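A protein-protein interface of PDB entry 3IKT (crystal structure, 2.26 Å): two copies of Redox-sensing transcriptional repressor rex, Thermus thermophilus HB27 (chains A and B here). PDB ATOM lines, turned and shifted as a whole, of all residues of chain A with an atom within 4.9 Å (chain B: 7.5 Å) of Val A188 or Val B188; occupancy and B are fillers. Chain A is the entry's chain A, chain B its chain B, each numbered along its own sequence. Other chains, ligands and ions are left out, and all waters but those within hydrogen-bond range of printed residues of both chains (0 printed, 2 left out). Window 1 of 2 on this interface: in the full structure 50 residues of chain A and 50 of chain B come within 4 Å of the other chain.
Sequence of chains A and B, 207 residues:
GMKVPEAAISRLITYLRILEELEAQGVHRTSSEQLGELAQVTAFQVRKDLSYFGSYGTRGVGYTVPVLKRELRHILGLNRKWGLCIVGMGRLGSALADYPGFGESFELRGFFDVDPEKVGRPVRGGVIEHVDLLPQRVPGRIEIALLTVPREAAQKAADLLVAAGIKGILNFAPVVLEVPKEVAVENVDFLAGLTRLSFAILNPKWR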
ATOM      1  N   LEU A 170      10.083  16.225 -18.189  1.00  0.00           N
ATOM      2  CA  LEU A 170      10.511  14.838 -18.169  1.00  0.00           C
ATOM      3  C   LEU A 170      11.161  14.740 -16.789  1.00  0.00           C
ATOM      4  O   LEU A 170      12.269  15.232 -16.574  1.00  0.00           O
ATOM      5  CB  LEU A 170      11.532  14.579 -19.270  1.00  0.00           C
ATOM      6  CG  LEU A 170      11.880  13.110 -19.526  1.00  0.00           C
ATOM      7  CD1 LEU A 170      10.639  12.315 -19.965  1.00  0.00           C
ATOM      8  CD2 LEU A 170      12.924  13.056 -20.605  1.00  0.00           C
ATOM      9  N   ASN A 171      10.439  14.121 -15.863  1.00  0.00           N
ATOM     10  CA  ASN A 171      10.854  13.983 -14.473  1.00  0.00           C
ATOM     11  C   ASN A 171      11.650  12.732 -14.119  1.00  0.00           C
ATOM     12  O   ASN A 171      11.125  11.626 -14.173  1.00  0.00           O
ATOM     13  CB  ASN A 171       9.607  14.053 -13.587  1.00  0.00           C
ATOM     14  CG  ASN A 171       9.918  13.829 -12.131  1.00  0.00           C
ATOM     15  OD1 ASN A 171      10.872  14.388 -11.598  1.00  0.00           O
ATOM     16  ND2 ASN A 171       9.102  13.017 -11.472  1.00  0.00           N
ATOM     17  N   PHE A 172      12.907  12.922 -13.731  1.00  0.00           N
ATOM     18  CA  PHE A 172      13.770  11.816 -13.342  1.00  0.00           C
ATOM     19  C   PHE A 172      13.807  11.605 -11.830  1.00  0.00           C
ATOM     20  O   PHE A 172      14.525  10.723 -11.348  1.00  0.00           O
ATOM     21  CB  PHE A 172      15.201  12.049 -13.836  1.00  0.00           C
ATOM     22  CG  PHE A 172      15.334  12.041 -15.329  1.00  0.00           C
ATOM     23  CD1 PHE A 172      14.998  13.170 -16.082  1.00  0.00           C
ATOM     24  CD2 PHE A 172      15.786  10.901 -15.987  1.00  0.00           C
ATOM     25  CE1 PHE A 172      15.110  13.161 -17.468  1.00  0.00           C
ATOM     26  CE2 PHE A 172      15.905  10.879 -17.380  1.00  0.00           C
ATOM     27  CZ  PHE A 172      15.565  12.016 -18.124  1.00  0.00           C
ATOM     28  N   GLU A 186       6.074  13.503 -17.809  1.00  0.00           N
ATOM     29  CA  GLU A 186       6.416  12.116 -18.090  1.00  0.00           C
ATOM     30  C   GLU A 186       7.530  11.729 -17.130  1.00  0.00           C
ATOM     31  O   GLU A 186       8.526  12.445 -17.015  1.00  0.00           O
ATOM     32  CB  GLU A 186       6.914  11.949 -19.528  1.00  0.00           C
ATOM     33  CG  GLU A 186       5.833  11.735 -20.562  1.00  0.00           C
ATOM     34  CD  GLU A 186       5.110  10.417 -20.363  1.00  0.00           C
ATOM     35  OE1 GLU A 186       5.784   9.373 -20.258  1.00  0.00           O
ATOM     36  OE2 GLU A 186       3.870  10.428 -20.305  1.00  0.00           O
ATOM     37  N   ASN A 187       7.377  10.600 -16.445  1.00  0.00           N
ATOM     38  CA  ASN A 187       8.414  10.159 -15.511  1.00  0.00           C
ATOM     39  C   ASN A 187       9.328   9.075 -16.079  1.00  0.00           C
ATOM     40  O   ASN A 187       8.874   8.179 -16.777  1.00  0.00           O
ATOM     41  CB  ASN A 187       7.787   9.613 -14.224  1.00  0.00           C
ATOM     42  CG  ASN A 187       6.893  10.616 -13.531  1.00  0.00           C
ATOM     43  OD1 ASN A 187       7.340  11.678 -13.091  1.00  0.00           O
ATOM     44  ND2 ASN A 187       5.612  10.280 -13.424  1.00  0.00           N
ATOM     45  N   VAL A 188      10.620   9.177 -15.781  1.00  0.00           N
ATOM     46  CA  VAL A 188      11.609   8.173 -16.175  1.00  0.00           C
ATOM     47  C   VAL A 188      12.124   7.840 -14.783  1.00  0.00           C
ATOM     48  O   VAL A 188      12.927   8.576 -14.202  1.00  0.00           O
ATOM     49  CB  VAL A 188      12.726   8.762 -17.058  1.00  0.00           C
ATOM     50  CG1 VAL A 188      13.743   7.684 -17.371  1.00  0.00           C
ATOM     51  CG2 VAL A 188      12.129   9.301 -18.360  1.00  0.00           C
ATOM     52  N   ASP A 189      11.643   6.722 -14.257  1.00  0.00           N
ATOM     53  CA  ASP A 189      11.903   6.321 -12.878  1.00  0.00           C
ATOM     54  C   ASP A 189      12.664   5.005 -12.787  1.00  0.00           C
ATOM     55  O   ASP A 189      12.064   3.935 -12.795  1.00  0.00           O
ATOM     56  CB  ASP A 189      10.519   6.216 -12.212  1.00  0.00           C
ATOM     57  CG  ASP A 189      10.574   6.178 -10.711  1.00  0.00           C
ATOM     58  OD1 ASP A 189       9.572   6.608 -10.099  1.00  0.00           O
ATOM     59  OD2 ASP A 189      11.581   5.711 -10.142  1.00  0.00           O
ATOM     60  N   PHE A 190      13.985   5.067 -12.681  1.00  0.00           N
ATOM     61  CA  PHE A 190      14.738   3.825 -12.635  1.00  0.00           C
ATOM     62  C   PHE A 190      14.602   3.062 -11.319  1.00  0.00           C
ATOM     63  O   PHE A 190      14.633   1.837 -11.327  1.00  0.00           O
ATOM     64  CB  PHE A 190      16.214   4.066 -13.014  1.00  0.00           C
ATOM     65  CG  PHE A 190      17.158   4.091 -11.852  1.00  0.00           C
ATOM     66  CD1 PHE A 190      17.384   5.261 -11.148  1.00  0.00           C
ATOM     67  CD2 PHE A 190      17.846   2.943 -11.478  1.00  0.00           C
ATOM     68  CE1 PHE A 190      18.288   5.294 -10.084  1.00  0.00           C
ATOM     69  CE2 PHE A 190      18.753   2.961 -10.414  1.00  0.00           C
ATOM     70  CZ  PHE A 190      18.973   4.141  -9.718  1.00  0.00           C
ATOM     71  N   GLY A 193      11.598   1.021 -11.663  1.00  0.00           N
ATOM     72  CA  GLY A 193      11.854  -0.117 -12.529  1.00  0.00           C
ATOM     73  C   GLY A 193      12.556  -1.220 -11.743  1.00  0.00           C
ATOM     74  O   GLY A 193      12.239  -2.399 -11.877  1.00  0.00           O
ATOM     75  N   LEU B  92      26.441   6.791 -18.182  1.00  0.00           N
ATOM     76  CA  LEU B  92      25.295   6.408 -17.363  1.00  0.00           C
ATOM     77  C   LEU B  92      25.723   5.391 -16.308  1.00  0.00           C
ATOM     78  O   LEU B  92      25.416   5.543 -15.122  1.00  0.00           O
ATOM     79  CB  LEU B  92      24.179   5.830 -18.243  1.00  0.00           C
ATOM     80  CG  LEU B  92      22.906   5.386 -17.514  1.00  0.00           C
ATOM     81  CD1 LEU B  92      22.388   6.514 -16.639  1.00  0.00           C
ATOM     82  CD2 LEU B  92      21.854   4.970 -18.528  1.00  0.00           C
ATOM     83  N   LEU B 147      21.438  -2.729 -17.469  1.00  0.00           N
ATOM     84  CA  LEU B 147      22.024  -2.718 -18.810  1.00  0.00           C
ATOM     85  C   LEU B 147      22.142  -1.310 -19.401  1.00  0.00           C
ATOM     86  O   LEU B 147      21.142  -0.710 -19.811  1.00  0.00           O
ATOM     87  CB  LEU B 147      21.209  -3.625 -19.737  1.00  0.00           C
ATOM     88  CG  LEU B 147      21.823  -4.011 -21.091  1.00  0.00           C
ATOM     89  CD1 LEU B 147      23.181  -4.653 -20.874  1.00  0.00           C
ATOM     90  CD2 LEU B 147      20.895  -4.972 -21.825  1.00  0.00           C
ATOM     91  N   ILE B 169      16.660  -7.974 -15.812  1.00  0.00           N
ATOM     92  CA  ILE B 169      17.367  -6.938 -16.534  1.00  0.00           C
ATOM     93  C   ILE B 169      16.630  -5.595 -16.514  1.00  0.00           C
ATOM     94  O   ILE B 169      15.475  -5.506 -16.932  1.00  0.00           O
ATOM     95  CB  ILE B 169      17.588  -7.346 -18.014  1.00  0.00           C
ATOM     96  CG1 ILE B 169      18.422  -8.633 -18.091  1.00  0.00           C
ATOM     97  CG2 ILE B 169      18.291  -6.217 -18.753  1.00  0.00           C
ATOM     98  CD1 ILE B 169      18.628  -9.154 -19.512  1.00  0.00           C
ATOM     99  N   LEU B 170      17.302  -4.567 -16.000  1.00  0.00           N
ATOM    100  CA  LEU B 170      16.751  -3.213 -15.989  1.00  0.00           C
ATOM    101  C   LEU B 170      17.389  -2.645 -17.253  1.00  0.00           C
ATOM    102  O   LEU B 170      18.572  -2.295 -17.258  1.00  0.00           O
ATOM    103  CB  LEU B 170      17.224  -2.433 -14.760  1.00  0.00           C
ATOM    104  CG  LEU B 170      16.573  -1.056 -14.546  1.00  0.00           C
ATOM    105  CD1 LEU B 170      15.102  -1.221 -14.193  1.00  0.00           C
ATOM    106  CD2 LEU B 170      17.287  -0.316 -13.432  1.00  0.00           C
ATOM    107  N   ASN B 171      16.597  -2.576 -18.320  1.00  0.00           N
ATOM    108  CA  ASN B 171      17.059  -2.129 -19.635  1.00  0.00           C
ATOM    109  C   ASN B 171      16.946  -0.632 -19.932  1.00  0.00           C
ATOM    110  O   ASN B 171      15.850  -0.073 -19.998  1.00  0.00           O
ATOM    111  CB  ASN B 171      16.314  -2.947 -20.710  1.00  0.00           C
ATOM    112  CG  ASN B 171      16.707  -2.566 -22.118  1.00  0.00           C
ATOM    113  OD1 ASN B 171      17.887  -2.372 -22.419  1.00  0.00           O
ATOM    114  ND2 ASN B 171      15.717  -2.468 -22.998  1.00  0.00           N
ATOM    115  N   PHE B 172      18.093   0.007 -20.132  1.00  0.00           N
ATOM    116  CA  PHE B 172      18.130   1.434 -20.426  1.00  0.00           C
ATOM    117  C   PHE B 172      18.278   1.706 -21.926  1.00  0.00           C
ATOM    118  O   PHE B 172      18.255   2.860 -22.349  1.00  0.00           O
ATOM    119  CB  PHE B 172      19.284   2.105 -19.675  1.00  0.00           C
ATOM    120  CG  PHE B 172      19.103   2.154 -18.185  1.00  0.00           C
ATOM    121  CD1 PHE B 172      19.459   1.071 -17.386  1.00  0.00           C
ATOM    122  CD2 PHE B 172      18.594   3.301 -17.575  1.00  0.00           C
ATOM    123  CE1 PHE B 172      19.317   1.130 -15.993  1.00  0.00           C
ATOM    124  CE2 PHE B 172      18.446   3.374 -16.187  1.00  0.00           C
ATOM    125  CZ  PHE B 172      18.810   2.283 -15.392  1.00  0.00           C
ATOM    126  N   ALA B 173      18.430   0.647 -22.721  1.00  0.00           N
ATOM    127  CA  ALA B 173      18.592   0.784 -24.167  1.00  0.00           C
ATOM    128  C   ALA B 173      17.241   0.793 -24.873  1.00  0.00           C
ATOM    129  O   ALA B 173      16.370  -0.024 -24.568  1.00  0.00           O
ATOM    130  CB  ALA B 173      19.455  -0.353 -24.706  1.00  0.00           C
ATOM    131  N   PRO B 174      17.060   1.711 -25.842  1.00  0.00           N
ATOM    132  CA  PRO B 174      15.843   1.902 -26.644  1.00  0.00           C
ATOM    133  C   PRO B 174      15.550   0.802 -27.661  1.00  0.00           C
ATOM    134  O   PRO B 174      15.487   1.050 -28.864  1.00  0.00           O
ATOM    135  CB  PRO B 174      16.087   3.253 -27.310  1.00  0.00           C
ATOM    136  CG  PRO B 174      17.554   3.216 -27.547  1.00  0.00           C
ATOM    137  CD  PRO B 174      18.081   2.702 -26.223  1.00  0.00           C
ATOM    138  N   GLU B 186      12.736  -5.028 -17.410  1.00  0.00           N
ATOM    139  CA  GLU B 186      12.016  -3.806 -17.112  1.00  0.00           C
ATOM    140  C   GLU B 186      12.785  -2.714 -17.838  1.00  0.00           C
ATOM    141  O   GLU B 186      14.003  -2.611 -17.701  1.00  0.00           O
ATOM    142  CB  GLU B 186      11.995  -3.550 -15.605  1.00  0.00           C
ATOM    143  CG  GLU B 186      11.119  -2.387 -15.205  1.00  0.00           C
ATOM    144  CD  GLU B 186       9.633  -2.681 -15.347  1.00  0.00           C
ATOM    145  OE1 GLU B 186       8.862  -1.711 -15.469  1.00  0.00           O
ATOM    146  OE2 GLU B 186       9.230  -3.864 -15.320  1.00  0.00           O
ATOM    147  N   ASN B 187      12.079  -1.918 -18.633  1.00  0.00           N
ATOM    148  CA  ASN B 187      12.723  -0.856 -19.390  1.00  0.00           C
ATOM    149  C   ASN B 187      12.616   0.517 -18.745  1.00  0.00           C
ATOM    150  O   ASN B 187      11.608   0.847 -18.131  1.00  0.00           O
ATOM    151  CB  ASN B 187      12.127  -0.758 -20.801  1.00  0.00           C
ATOM    152  CG  ASN B 187      12.280  -2.043 -21.605  1.00  0.00           C
ATOM    153  OD1 ASN B 187      13.380  -2.565 -21.765  1.00  0.00           O
ATOM    154  ND2 ASN B 187      11.163  -2.549 -22.129  1.00  0.00           N
ATOM    155  N   VAL B 188      13.682   1.299 -18.879  1.00  0.00           N
ATOM    156  CA  VAL B 188      13.722   2.681 -18.397  1.00  0.00           C
ATOM    157  C   VAL B 188      14.146   3.342 -19.704  1.00  0.00           C
ATOM    158  O   VAL B 188      15.282   3.197 -20.156  1.00  0.00           O
ATOM    159  CB  VAL B 188      14.762   2.875 -17.288  1.00  0.00           C
ATOM    160  CG1 VAL B 188      14.787   4.334 -16.845  1.00  0.00           C
ATOM    161  CG2 VAL B 188      14.408   1.989 -16.103  1.00  0.00           C
ATOM    162  N   ASP B 189      13.199   4.043 -20.317  1.00  0.00           N
ATOM    163  CA  ASP B 189      13.382   4.625 -21.641  1.00  0.00           C
ATOM    164  C   ASP B 189      13.142   6.127 -21.653  1.00  0.00           C
ATOM    165  O   ASP B 189      12.006   6.573 -21.828  1.00  0.00           O
ATOM    166  CB  ASP B 189      12.384   3.907 -22.552  1.00  0.00           C
ATOM    167  CG  ASP B 189      12.705   4.034 -24.019  1.00  0.00           C
ATOM    168  OD1 ASP B 189      12.301   3.111 -24.753  1.00  0.00           O
ATOM    169  OD2 ASP B 189      13.324   5.036 -24.442  1.00  0.00           O
ATOM    170  N   PHE B 190      14.204   6.912 -21.488  1.00  0.00           N
ATOM    171  CA  PHE B 190      14.037   8.357 -21.450  1.00  0.00           C
ATOM    172  C   PHE B 190      13.666   8.940 -22.815  1.00  0.00           C
ATOM    173  O   PHE B 190      12.928   9.922 -22.887  1.00  0.00           O
ATOM    174  CB  PHE B 190      15.291   9.024 -20.835  1.00  0.00           C
ATOM    175  CG  PHE B 190      16.264   9.577 -21.836  1.00  0.00           C
ATOM    176  CD1 PHE B 190      16.089  10.856 -22.366  1.00  0.00           C
ATOM    177  CD2 PHE B 190      17.362   8.834 -22.236  1.00  0.00           C
ATOM    178  CE1 PHE B 190      16.998  11.385 -23.277  1.00  0.00           C
ATOM    179  CE2 PHE B 190      18.279   9.355 -23.151  1.00  0.00           C
ATOM    180  CZ  PHE B 190      18.095  10.634 -23.671  1.00  0.00           C
ATOM    181  N   LEU B 191      14.138   8.325 -23.897  1.00  0.00           N
ATOM    182  CA  LEU B 191      13.783   8.807 -25.230  1.00  0.00           C
ATOM    183  C   LEU B 191      12.281   8.617 -25.477  1.00  0.00           C
ATOM    184  O   LEU B 191      11.620   9.490 -26.040  1.00  0.00           O
ATOM    185  CB  LEU B 191      14.594   8.081 -26.307  1.00  0.00           C
ATOM    186  CG  LEU B 191      16.048   8.553 -26.423  1.00  0.00           C
ATOM    187  CD1 LEU B 191      16.834   7.686 -27.416  1.00  0.00           C
ATOM    188  CD2 LEU B 191      16.050  10.005 -26.868  1.00  0.00           C
ATOM    189  N   ALA B 192      11.735   7.481 -25.048  1.00  0.00           N
ATOM    190  CA  ALA B 192      10.308   7.242 -25.229  1.00  0.00           C
ATOM    191  C   ALA B 192       9.552   8.288 -24.422  1.00  0.00           C
ATOM    192  O   ALA B 192       8.569   8.856 -24.898  1.00  0.00           O
ATOM    193  CB  ALA B 192       9.933   5.823 -24.762  1.00  0.00           C
ATOM    194  N   GLY B 193      10.029   8.544 -23.200  1.00  0.00           N
ATOM    195  CA  GLY B 193       9.406   9.535 -22.337  1.00  0.00           C
ATOM    196  C   GLY B 193       9.363  10.894 -23.014  1.00  0.00           C
ATOM    197  O   GLY B 193       8.354  11.596 -22.942  1.00  0.00           O
ATOM    198  N   LEU B 194      10.469  11.266 -23.659  1.00  0.00           N
ATOM    199  CA  LEU B 194      10.560  12.525 -24.403  1.00  0.00           C
ATOM    200  C   LEU B 194       9.542  12.570 -25.542  1.00  0.00           C
ATOM    201  O   LEU B 194       8.834  13.560 -25.715  1.00  0.00           O
ATOM    202  CB  LEU B 194      11.945  12.691 -25.029  1.00  0.00           C
ATOM    203  CG  LEU B 194      13.072  13.345 -24.245  1.00  0.00           C
ATOM    204  CD1 LEU B 194      14.288  13.509 -25.171  1.00  0.00           C
ATOM    205  CD2 LEU B 194      12.598  14.700 -23.727  1.00  0.00           C
ATOM    206  N   ARG B 196       6.849  10.877 -25.813  1.00  0.00           N
ATOM    207  CA  ARG B 196       5.493  10.937 -25.282  1.00  0.00           C
ATOM    208  C   ARG B 196       5.132  12.376 -24.920  1.00  0.00           C
ATOM    209  O   ARG B 196       3.984  12.785 -25.084  1.00  0.00           O
ATOM    210  CB  ARG B 196       5.334  10.025 -24.061  1.00  0.00           C
ATOM    211  CG  ARG B 196       5.320   8.539 -24.427  1.00  0.00           C
ATOM    212  CD  ARG B 196       4.648   7.710 -23.356  1.00  0.00           C
ATOM    213  NE  ARG B 196       5.389   7.738 -22.106  1.00  0.00           N
ATOM    214  CZ  ARG B 196       6.541   7.106 -21.913  1.00  0.00           C
ATOM    215  NH1 ARG B 196       7.075   6.393 -22.893  1.00  0.00           N
ATOM    216  NH2 ARG B 196       7.163   7.193 -20.748  1.00  0.00           N
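Of chain B, only Val B188 (3.5 Å) and Phe B190 (3.8 Å) come within 4 Å of Val A188.
Printed residues of chain A within 4 Å of Val B188: Val A188 and Phe A190.
Printed residues of chain B within 4 Å of Gly A193: Leu B170 (3.5 Å) and Glu B186 (3.5 Å).
Of the printed residues of chain A, Arg B196 touches Glu A186 (2.5 Å).
Asn B187 touches none of the printed residues of chain A.
The nearest residue of chain A that does not touch Val B188 is Asp A189 (4.5 Å).
The nearest printed residue of chain B that does not touch Gly A193 is Val B188 (4.9 Å).
OE1 of Glu A186 is in salt-bridge range of NE of Arg B196.
Of the 9 printed residues of chain A, 6 touch a printed residue of chain B.
Hydrophobic or aromatic side chains of chain B that line the printed part of chain A: Leu B170, Phe B172, Val B188, Phe B190 and Leu B194.
Among the printed residues, 13 pairs touch across the chains.
O of Asn A171 is in hydrogen-bond range of N of Val A188.
The backbone NH of Leu B147 lies within hydrogen-bond range of the backbone carbonyl oxygen of Leu B170.
O of Leu B147 is in hydrogen-bond range of N of Phe B172 (3.1 Å).
The backbone NH (N) of Glu B186 lies within hydrogen-bond range of the backbone carbonyl oxygen (O) of Ile B169, 2.8 Å away.
The backbone NH of Asn B171 sits at hydrogen-bond distance from the backbone carbonyl oxygen of Glu B186.
The backbone NH (N) of Val B188 is in hydrogen-bond range of the backbone carbonyl oxygen (O) of Asn B171 (2.8 Å).
Among the printed residues, merely in contact across the chains: Leu A170 with Phe B190, Leu A170 with Gly B193, Leu A170 with Leu B194, Phe A172 with Phe B190, Glu A186 with Gly B193, Val A188 with Val B188, Val A188 with Phe B190, Phe A190 with Leu B170, Phe A190 with Phe B172, Phe A190 with Val B188, Gly A193 with Leu B170 and Gly A193 with Glu B186.
Leu A170 touches Phe B190, and with the chains exchanged Phe A190 touches Leu B170.
Leu A170 touches Gly B193, and with the chains exchanged Gly A193 touches Leu B170.
Val A188 touches its own counterpart, Val B188.
Val A188 touches Phe B190, and with the chains exchanged Phe A190 touches Val B188.
Of the 13 pairs that touch across the chains among the printed residues, 11 have their exchanged pair printed and touching as well.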
